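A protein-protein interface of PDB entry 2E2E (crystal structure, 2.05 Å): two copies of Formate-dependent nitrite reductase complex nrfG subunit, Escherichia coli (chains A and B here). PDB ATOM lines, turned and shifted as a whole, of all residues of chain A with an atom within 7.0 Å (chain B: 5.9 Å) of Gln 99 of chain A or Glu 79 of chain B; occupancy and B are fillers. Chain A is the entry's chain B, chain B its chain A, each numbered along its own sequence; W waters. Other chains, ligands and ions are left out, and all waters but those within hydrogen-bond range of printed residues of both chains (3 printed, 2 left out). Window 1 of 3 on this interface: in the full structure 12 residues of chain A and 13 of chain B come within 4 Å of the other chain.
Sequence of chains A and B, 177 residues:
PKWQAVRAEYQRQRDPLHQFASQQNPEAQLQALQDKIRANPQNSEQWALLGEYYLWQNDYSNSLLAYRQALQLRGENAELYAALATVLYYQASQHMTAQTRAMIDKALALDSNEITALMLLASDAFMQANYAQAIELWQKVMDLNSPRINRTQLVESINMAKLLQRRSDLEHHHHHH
Among the printed residues, pairs that only touch across the chains: Ala 92 of chain A with Asn 77 of chain B (3.5 Å), Thr 97 of chain A with Glu 79 of chain B (3.5 Å), Thr 97 of chain A with Arg 74 of chain B (3.6 Å), Met 96 of chain A with Arg 74 of chain B (3.7 Å) and Thr 97 of chain A with Glu 45 of chain B (3.9 Å).
The side-chain carboxylate of Glu 45 of chain B lies within hydrogen-bond range of the backbone NH of Ala 98 of chain A (2.9 Å). The side-chain amide oxygen of Gln 99 of chain A sits at hydrogen-bond distance from the side-chain amide nitrogen of Gln 13 of chain B. NE2 of Gln 99 of chain A is in hydrogen-bond range of OE2 of Glu 79 of chain B, 2.9 Å away.
OD1 of Asn 77 of chain B is in hydrogen-bond range of N of Leu 80 of chain B (3.1 Å). OD1 of Asn 77 of chain B sits close to N of Glu 79 of chain B. The side-chain carboxylate of Glu 45 of chain B is in salt-bridge range of the guanidinium group of Arg 74 of chain B, 2.5 Å away.
Of the 15 printed residues of chain A, 5 touch a printed residue of chain B. Printed residues of chain A that touch a printed residue of chain B: Ala 92, Met 96, Thr 97, Ala 98 and Gln 99. Hydrophobic or aromatic side chains of chain A that line the printed part of chain B: Ala 92 and Ala 98. Among the printed residues, no Asp or Glu carboxylate lies within 4 Å of a Lys or Arg side-chain nitrogen of the other chain.
Water W2 lies within hydrogen-bond range of O of Ala 92 of chain A and ND2 of Asn 77 of chain B. Water W1 lies within hydrogen-bond range of N of Gln 99 of chain A (3.0 Å), OE2 of Glu 79 of chain B (3.1 Å), OE1 of Glu 45 of chain B (3.2 Å) and N of Ala 98 of chain A (3.4 Å). Water W3 lies within hydrogen-bond range of the backbone carbonyl oxygen (O) of Gln 91 of chain A (3.0 Å) and the backbone NH (N) of Ala 78 of chain B (3.2 Å).
Gln 99 of chain A touches just these residues of chain B: Gln 13 and Glu 79. Of the printed residues of chain A, Glu 79 of chain B touches Thr 97 and Gln 99. Printed residues of chain A within 4 Å of Arg 74 of chain B: Met 96 and Thr 97. Of the printed residues of chain A, Asn 77 of chain B touches Ala 92.
Position printed for both chains: 84. Of the 8 pairs that touch across the chains among the printed residues, none has its exchanged pair printed and touching as well.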
ATOM      1  N   LEU A  64      30.290  -3.727  10.980  1.00  0.00           N
ATOM      2  CA  LEU A  64      31.132  -4.737  11.633  1.00  0.00           C
ATOM      3  C   LEU A  64      32.364  -5.075  10.819  1.00  0.00           C
ATOM      4  O   LEU A  64      33.466  -5.217  11.384  1.00  0.00           O
ATOM      5  CB  LEU A  64      30.348  -6.026  11.932  1.00  0.00           C
ATOM      6  CG  LEU A  64      29.364  -5.952  13.095  1.00  0.00           C
ATOM      7  CD1 LEU A  64      28.458  -7.211  13.126  1.00  0.00           C
ATOM      8  CD2 LEU A  64      30.084  -5.739  14.451  1.00  0.00           C
ATOM      9  N   LEU A  84      32.811  -1.786  18.181  1.00  0.00           N
ATOM     10  CA  LEU A  84      32.331  -3.131  17.895  1.00  0.00           C
ATOM     11  C   LEU A  84      31.169  -3.525  18.796  1.00  0.00           C
ATOM     12  O   LEU A  84      30.143  -4.013  18.306  1.00  0.00           O
ATOM     13  CB  LEU A  84      33.476  -4.141  18.063  1.00  0.00           C
ATOM     14  CG  LEU A  84      34.152  -4.786  16.846  1.00  0.00           C
ATOM     15  CD1 LEU A  84      33.704  -4.241  15.493  1.00  0.00           C
ATOM     16  CD2 LEU A  84      35.677  -4.764  16.969  1.00  0.00           C
ATOM     17  N   ALA A  85      31.311  -3.253  20.095  1.00  0.00           N
ATOM     18  CA  ALA A  85      30.280  -3.624  21.065  1.00  0.00           C
ATOM     19  C   ALA A  85      29.033  -2.842  20.792  1.00  0.00           C
ATOM     20  O   ALA A  85      27.948  -3.377  20.851  1.00  0.00           O
ATOM     21  CB  ALA A  85      30.755  -3.347  22.478  1.00  0.00           C
ATOM     22  N   LEU A  88      27.387  -4.530  17.626  1.00  0.00           N
ATOM     23  CA  LEU A  88      26.798  -5.793  18.050  1.00  0.00           C
ATOM     24  C   LEU A  88      25.503  -5.586  18.861  1.00  0.00           C
ATOM     25  O   LEU A  88      24.478  -6.205  18.600  1.00  0.00           O
ATOM     26  CB  LEU A  88      27.845  -6.552  18.880  1.00  0.00           C
ATOM     27  CG  LEU A  88      28.999  -7.142  18.057  1.00  0.00           C
ATOM     28  CD1 LEU A  88      30.078  -7.764  18.966  1.00  0.00           C
ATOM     29  CD2 LEU A  88      28.498  -8.177  17.060  1.00  0.00           C
ATOM     30  N   GLN A  91      22.804  -4.234  16.550  1.00  0.00           N
ATOM     31  CA  GLN A  91      22.457  -5.358  15.699  1.00  0.00           C
ATOM     32  C   GLN A  91      21.532  -6.366  16.369  1.00  0.00           C
ATOM     33  O   GLN A  91      20.678  -6.969  15.694  1.00  0.00           O
ATOM     34  CB  GLN A  91      23.721  -6.064  15.231  1.00  0.00           C
ATOM     35  CG  GLN A  91      23.476  -7.152  14.171  1.00  0.00           C
ATOM     36  CD  GLN A  91      24.725  -7.884  13.872  1.00  0.00           C
ATOM     37  OE1 GLN A  91      25.126  -7.982  12.726  1.00  0.00           O
ATOM     38  NE2 GLN A  91      25.390  -8.358  14.910  1.00  0.00           N
ATOM     39  N   ALA A  92      21.714  -6.566  17.678  1.00  0.00           N
ATOM     40  CA  ALA A  92      20.850  -7.422  18.459  1.00  0.00           C
ATOM     41  C   ALA A  92      19.675  -6.636  19.033  1.00  0.00           C
ATOM     42  O   ALA A  92      19.208  -6.969  20.123  1.00  0.00           O
ATOM     43  CB  ALA A  92      21.635  -8.077  19.629  1.00  0.00           C
ATOM     44  N   MET A  96      21.676  -7.320  25.256  1.00  0.00           N
ATOM     45  CA  MET A  96      23.013  -7.797  25.523  1.00  0.00           C
ATOM     46  C   MET A  96      23.140  -9.160  24.899  1.00  0.00           C
ATOM     47  O   MET A  96      22.138  -9.855  24.663  1.00  0.00           O
ATOM     48  CB  MET A  96      23.333  -7.869  27.032  1.00  0.00           C
ATOM     49  CG  MET A  96      24.840  -8.003  27.390  1.00  0.00           C
ATOM     50  SD  MET A  96      26.009  -6.828  26.640  1.00  0.00           S
ATOM     51  CE  MET A  96      25.583  -5.273  27.432  1.00  0.00           C
ATOM     52  N   THR A  97      24.384  -9.549  24.675  1.00  0.00           N
ATOM     53  CA  THR A  97      24.718 -10.666  23.855  1.00  0.00           C
ATOM     54  C   THR A  97      26.091 -11.050  24.392  1.00  0.00           C
ATOM     55  O   THR A  97      26.798 -10.200  24.947  1.00  0.00           O
ATOM     56  CB  THR A  97      24.733 -10.162  22.363  1.00  0.00           C
ATOM     57  OG1 THR A  97      23.729 -10.828  21.600  1.00  0.00           O
ATOM     58  CG2 THR A  97      26.033 -10.303  21.703  1.00  0.00           C
ATOM     59  N   ALA A  98      26.441 -12.324  24.291  1.00  0.00           N
ATOM     60  CA  ALA A  98      27.776 -12.784  24.656  1.00  0.00           C
ATOM     61  C   ALA A  98      28.880 -12.083  23.839  1.00  0.00           C
ATOM     62  O   ALA A  98      29.874 -11.647  24.409  1.00  0.00           O
ATOM     63  CB  ALA A  98      27.877 -14.316  24.523  1.00  0.00           C
ATOM     64  N   GLN A  99      28.712 -11.965  22.521  1.00  0.00           N
ATOM     65  CA  GLN A  99      29.682 -11.209  21.703  1.00  0.00           C
ATOM     66  C   GLN A  99      29.814  -9.769  22.205  1.00  0.00           C
ATOM     67  O   GLN A  99      30.913  -9.227  22.277  1.00  0.00           O
ATOM     68  CB  GLN A  99      29.250 -11.143  20.229  1.00  0.00           C
ATOM     69  CG  GLN A  99      29.309 -12.418  19.421  1.00  0.00           C
ATOM     70  CD  GLN A  99      29.176 -12.112  17.929  1.00  0.00           C
ATOM     71  OE1 GLN A  99      30.189 -11.988  17.209  1.00  0.00           O
ATOM     72  NE2 GLN A  99      27.934 -11.953  17.463  1.00  0.00           N
ATOM     73  N   THR A 100      28.675  -9.137  22.493  1.00  0.00           N
ATOM     74  CA  THR A 100      28.661  -7.761  22.944  1.00  0.00           C
ATOM     75  C   THR A 100      29.418  -7.636  24.262  1.00  0.00           C
ATOM     76  O   THR A 100      30.256  -6.747  24.397  1.00  0.00           O
ATOM     77  CB  THR A 100      27.234  -7.157  23.051  1.00  0.00           C
ATOM     78  OG1 THR A 100      26.526  -7.343  21.817  1.00  0.00           O
ATOM     79  CG2 THR A 100      27.296  -5.654  23.361  1.00  0.00           C
ATOM     80  N   ARG A 101      29.151  -8.523  25.226  1.00  0.00           N
ATOM     81  CA  ARG A 101      29.742  -8.345  26.536  1.00  0.00           C
ATOM     82  C   ARG A 101      31.244  -8.550  26.481  1.00  0.00           C
ATOM     83  O   ARG A 101      31.968  -7.903  27.236  1.00  0.00           O
ATOM     84  CB  ARG A 101      29.128  -9.255  27.586  1.00  0.00           C
ATOM     85  CG  ARG A 101      29.615  -8.931  28.973  1.00  0.00           C
ATOM     86  CD  ARG A 101      28.806  -9.631  30.032  1.00  0.00           C
ATOM     87  NE  ARG A 101      27.439  -9.117  30.069  1.00  0.00           N
ATOM     88  CZ  ARG A 101      27.042  -8.064  30.781  1.00  0.00           C
ATOM     89  NH1 ARG A 101      27.913  -7.391  31.529  1.00  0.00           N
ATOM     90  NH2 ARG A 101      25.770  -7.692  30.739  1.00  0.00           N
ATOM     91  N   ALA A 102      31.710  -9.434  25.591  1.00  0.00           N
ATOM     92  CA  ALA A 102      33.138  -9.702  25.489  1.00  0.00           C
ATOM     93  C   ALA A 102      33.876  -8.523  24.852  1.00  0.00           C
ATOM     94  O   ALA A 102      34.975  -8.202  25.272  1.00  0.00           O
ATOM     95  CB  ALA A 102      33.435 -11.027  24.746  1.00  0.00           C
ATOM     96  N   MET A 103      33.277  -7.868  23.861  1.00  0.00           N
ATOM     97  CA  MET A 103      33.890  -6.641  23.303  1.00  0.00           C
ATOM     98  C   MET A 103      33.981  -5.525  24.348  1.00  0.00           C
ATOM     99  O   MET A 103      34.957  -4.765  24.358  1.00  0.00           O
ATOM    100  CB  MET A 103      33.170  -6.141  22.046  1.00  0.00           C
ATOM    101  CG  MET A 103      33.260  -7.027  20.800  1.00  0.00           C
ATOM    102  SD  MET A 103      34.920  -7.416  20.153  1.00  0.00           S
ATOM    103  CE  MET A 103      35.319  -8.847  21.145  1.00  0.00           C
ATOM    104  N   ILE A 104      32.969  -5.435  25.212  1.00  0.00           N
ATOM    105  CA  ILE A 104      32.927  -4.465  26.327  1.00  0.00           C
ATOM    106  C   ILE A 104      34.007  -4.790  27.381  1.00  0.00           C
ATOM    107  O   ILE A 104      34.693  -3.888  27.912  1.00  0.00           O
ATOM    108  CB  ILE A 104      31.512  -4.404  26.971  1.00  0.00           C
ATOM    109  CG1 ILE A 104      30.526  -3.679  26.043  1.00  0.00           C
ATOM    110  CG2 ILE A 104      31.519  -3.659  28.299  1.00  0.00           C
ATOM    111  CD1 ILE A 104      29.055  -3.608  26.582  1.00  0.00           C
ATOM    112  N   GLN B  13      34.229 -19.380  17.206  1.00  0.00           N
ATOM    113  CA  GLN B  13      33.069 -18.883  17.964  1.00  0.00           C
ATOM    114  C   GLN B  13      32.079 -19.981  18.399  1.00  0.00           C
ATOM    115  O   GLN B  13      31.275 -19.737  19.285  1.00  0.00           O
ATOM    116  CB  GLN B  13      32.365 -17.692  17.298  1.00  0.00           C
ATOM    117  CG  GLN B  13      31.649 -16.759  18.306  1.00  0.00           C
ATOM    118  CD  GLN B  13      30.479 -15.964  17.709  1.00  0.00           C
ATOM    119  OE1 GLN B  13      29.305 -16.243  17.997  1.00  0.00           O
ATOM    120  NE2 GLN B  13      30.798 -14.967  16.888  1.00  0.00           N
ATOM    121  N   GLU B  45      19.979 -14.122  26.569  1.00  0.00           N
ATOM    122  CA  GLU B  45      21.181 -14.928  26.340  1.00  0.00           C
ATOM    123  C   GLU B  45      21.278 -16.125  27.314  1.00  0.00           C
ATOM    124  O   GLU B  45      21.948 -17.113  27.020  1.00  0.00           O
ATOM    125  CB  GLU B  45      22.439 -14.021  26.344  1.00  0.00           C
ATOM    126  CG  GLU B  45      23.706 -14.590  25.715  1.00  0.00           C
ATOM    127  CD  GLU B  45      23.785 -14.483  24.172  1.00  0.00           C
ATOM    128  OE1 GLU B  45      24.887 -14.657  23.644  1.00  0.00           O
ATOM    129  OE2 GLU B  45      22.781 -14.263  23.469  1.00  0.00           O
ATOM    130  N   ARG B  74      13.836 -11.647  22.938  1.00  0.00           N
ATOM    131  CA  ARG B  74      14.747 -10.738  22.235  1.00  0.00           C
ATOM    132  C   ARG B  74      14.116 -10.051  21.036  1.00  0.00           C
ATOM    133  O   ARG B  74      14.555  -8.957  20.622  1.00  0.00           O
ATOM    134  CB  ARG B  74      16.015 -11.482  21.763  1.00  0.00           C
ATOM    135  CG  ARG B  74      17.186 -10.540  21.488  1.00  0.00           C
ATOM    136  CD  ARG B  74      18.511 -11.240  21.219  1.00  0.00           C
ATOM    137  NE  ARG B  74      19.095 -11.789  22.434  1.00  0.00           N
ATOM    138  CZ  ARG B  74      20.164 -12.581  22.465  1.00  0.00           C
ATOM    139  NH1 ARG B  74      20.810 -12.911  21.350  1.00  0.00           N
ATOM    140  NH2 ARG B  74      20.604 -13.028  23.623  1.00  0.00           N
ATOM    141  N   ASN B  77      16.193 -11.819  15.703  1.00  0.00           N
ATOM    142  CA  ASN B  77      17.617 -11.727  15.953  1.00  0.00           C
ATOM    143  C   ASN B  77      18.312 -12.817  15.179  1.00  0.00           C
ATOM    144  O   ASN B  77      18.039 -14.001  15.426  1.00  0.00           O
ATOM    145  CB  ASN B  77      17.900 -11.884  17.452  1.00  0.00           C
ATOM    146  CG  ASN B  77      19.389 -11.949  17.767  1.00  0.00           C
ATOM    147  OD1 ASN B  77      19.958 -13.037  17.892  1.00  0.00           O
ATOM    148  ND2 ASN B  77      20.033 -10.780  17.879  1.00  0.00           N
ATOM    149  N   ALA B  78      19.212 -12.409  14.273  1.00  0.00           N
ATOM    150  CA  ALA B  78      19.898 -13.295  13.353  1.00  0.00           C
ATOM    151  C   ALA B  78      20.611 -14.490  13.977  1.00  0.00           C
ATOM    152  O   ALA B  78      20.462 -15.602  13.468  1.00  0.00           O
ATOM    153  CB  ALA B  78      20.862 -12.515  12.465  1.00  0.00           C
ATOM    154  N   GLU B  79      21.385 -14.266  15.052  1.00  0.00           N
ATOM    155  CA  GLU B  79      22.113 -15.355  15.754  1.00  0.00           C
ATOM    156  C   GLU B  79      21.175 -16.406  16.281  1.00  0.00           C
ATOM    157  O   GLU B  79      21.517 -17.569  16.285  1.00  0.00           O
ATOM    158  CB  GLU B  79      22.904 -14.847  16.967  1.00  0.00           C
ATOM    159  CG  GLU B  79      24.139 -14.064  16.658  1.00  0.00           C
ATOM    160  CD  GLU B  79      24.746 -13.488  17.935  1.00  0.00           C
ATOM    161  OE1 GLU B  79      24.061 -12.688  18.629  1.00  0.00           O
ATOM    162  OE2 GLU B  79      25.920 -13.838  18.224  1.00  0.00           O
ATOM    163  N   LEU B  80      20.026 -15.983  16.790  1.00  0.00           N
ATOM    164  CA  LEU B  80      19.026 -16.923  17.314  1.00  0.00           C
ATOM    165  C   LEU B  80      18.222 -17.610  16.211  1.00  0.00           C
ATOM    166  O   LEU B  80      17.925 -18.792  16.306  1.00  0.00           O
ATOM    167  CB  LEU B  80      18.084 -16.240  18.303  1.00  0.00           C
ATOM    168  CG  LEU B  80      18.753 -15.728  19.579  1.00  0.00           C
ATOM    169  CD1 LEU B  80      17.825 -14.732  20.247  1.00  0.00           C
ATOM    170  CD2 LEU B  80      19.083 -16.884  20.515  1.00  0.00           C
ATOM    171  N   TYR B  81      17.874 -16.878  15.159  1.00  0.00           N
ATOM    172  CA  TYR B  81      17.354 -17.515  13.956  1.00  0.00           C
ATOM    173  C   TYR B  81      18.265 -18.617  13.384  1.00  0.00           C
ATOM    174  O   TYR B  81      17.783 -19.650  12.942  1.00  0.00           O
ATOM    175  CB  TYR B  81      17.049 -16.464  12.884  1.00  0.00           C
ATOM    176  CG  TYR B  81      15.753 -15.697  13.107  1.00  0.00           C
ATOM    177  CD1 TYR B  81      15.660 -14.348  12.769  1.00  0.00           C
ATOM    178  CD2 TYR B  81      14.621 -16.318  13.657  1.00  0.00           C
ATOM    179  CE1 TYR B  81      14.474 -13.632  12.971  1.00  0.00           C
ATOM    180  CE2 TYR B  81      13.415 -15.607  13.861  1.00  0.00           C
ATOM    181  CZ  TYR B  81      13.359 -14.267  13.513  1.00  0.00           C
ATOM    182  OH  TYR B  81      12.196 -13.556  13.686  1.00  0.00           O
ATOM    183  N   ALA B  82      19.574 -18.355  13.359  1.00  0.00           N
ATOM    184  CA  ALA B  82      20.589 -19.286  12.888  1.00  0.00           C
ATOM    185  C   ALA B  82      20.762 -20.502  13.808  1.00  0.00           C
ATOM    186  O   ALA B  82      21.074 -21.597  13.340  1.00  0.00           O
ATOM    187  CB  ALA B  82      21.934 -18.555  12.721  1.00  0.00           C
ATOM    188  N   ALA B  83      20.570 -20.295  15.105  1.00  0.00           N
ATOM    189  CA  ALA B  83      20.695 -21.356  16.099  1.00  0.00           C
ATOM    190  C   ALA B  83      19.492 -22.288  16.025  1.00  0.00           C
ATOM    191  O   ALA B  83      19.650 -23.497  15.921  1.00  0.00           O
ATOM    192  CB  ALA B  83      20.828 -20.778  17.469  1.00  0.00           C
ATOM    193  N   LEU B  84      18.296 -21.723  16.035  1.00  0.00           N
ATOM    194  CA  LEU B  84      17.080 -22.466  15.698  1.00  0.00           C
ATOM    195  C   LEU B  84      17.242 -23.319  14.438  1.00  0.00           C
ATOM    196  O   LEU B  84      16.894 -24.517  14.437  1.00  0.00           O
ATOM    197  CB  LEU B  84      15.913 -21.488  15.510  1.00  0.00           C
ATOM    198  CG  LEU B  84      14.818 -21.345  16.574  1.00  0.00           C
ATOM    199  CD1 LEU B  84      15.064 -22.119  17.867  1.00  0.00           C
ATOM    200  CD2 LEU B  84      14.518 -19.875  16.866  1.00  0.00           C
ATOM    201  N   ALA B 107      17.238 -15.299   9.512  1.00  0.00           N
ATOM    202  CA  ALA B 107      18.594 -14.943   9.948  1.00  0.00           C
ATOM    203  C   ALA B 107      19.290 -14.011   8.976  1.00  0.00           C
ATOM    204  O   ALA B 107      19.841 -12.989   9.381  1.00  0.00           O
ATOM    205  CB  ALA B 107      19.455 -16.200  10.148  1.00  0.00           C
ATOM    206  N   GLU B 114      25.698 -13.588   8.505  1.00  0.00           N
ATOM    207  CA  GLU B 114      25.578 -14.480   9.646  1.00  0.00           C
ATOM    208  C   GLU B 114      26.174 -15.818   9.250  1.00  0.00           C
ATOM    209  O   GLU B 114      25.624 -16.522   8.410  1.00  0.00           O
ATOM    210  CB  GLU B 114      24.117 -14.632  10.058  1.00  0.00           C
ATOM    211  CG  GLU B 114      23.887 -14.745  11.576  1.00  0.00           C
ATOM    212  CD  GLU B 114      24.501 -15.984  12.195  1.00  0.00           C
ATOM    213  OE1 GLU B 114      24.558 -17.007  11.511  1.00  0.00           O
ATOM    214  OE2 GLU B 114      24.916 -15.960  13.366  1.00  0.00           O
ATOM    215  N   THR B 116      26.905 -18.718  10.853  1.00  0.00           N
ATOM    216  CA  THR B 116      26.226 -19.923  11.226  1.00  0.00           C
ATOM    217  C   THR B 116      25.200 -20.286  10.141  1.00  0.00           C
ATOM    218  O   THR B 116      25.160 -21.429   9.698  1.00  0.00           O
ATOM    219  CB  THR B 116      25.569 -19.796  12.626  1.00  0.00           C
ATOM    220  OG1 THR B 116      26.575 -19.498  13.609  1.00  0.00           O
ATOM    221  CG2 THR B 116      24.851 -21.094  12.996  1.00  0.00           C
HETATM  222  O   HOH W   1      26.695 -13.684  21.198  1.00  0.00           O
HETATM  223  O   HOH W   2      18.279  -9.095  19.098  1.00  0.00           O
HETATM  224  O   HOH W   3      20.383  -9.456  14.039  1.00  0.00           O
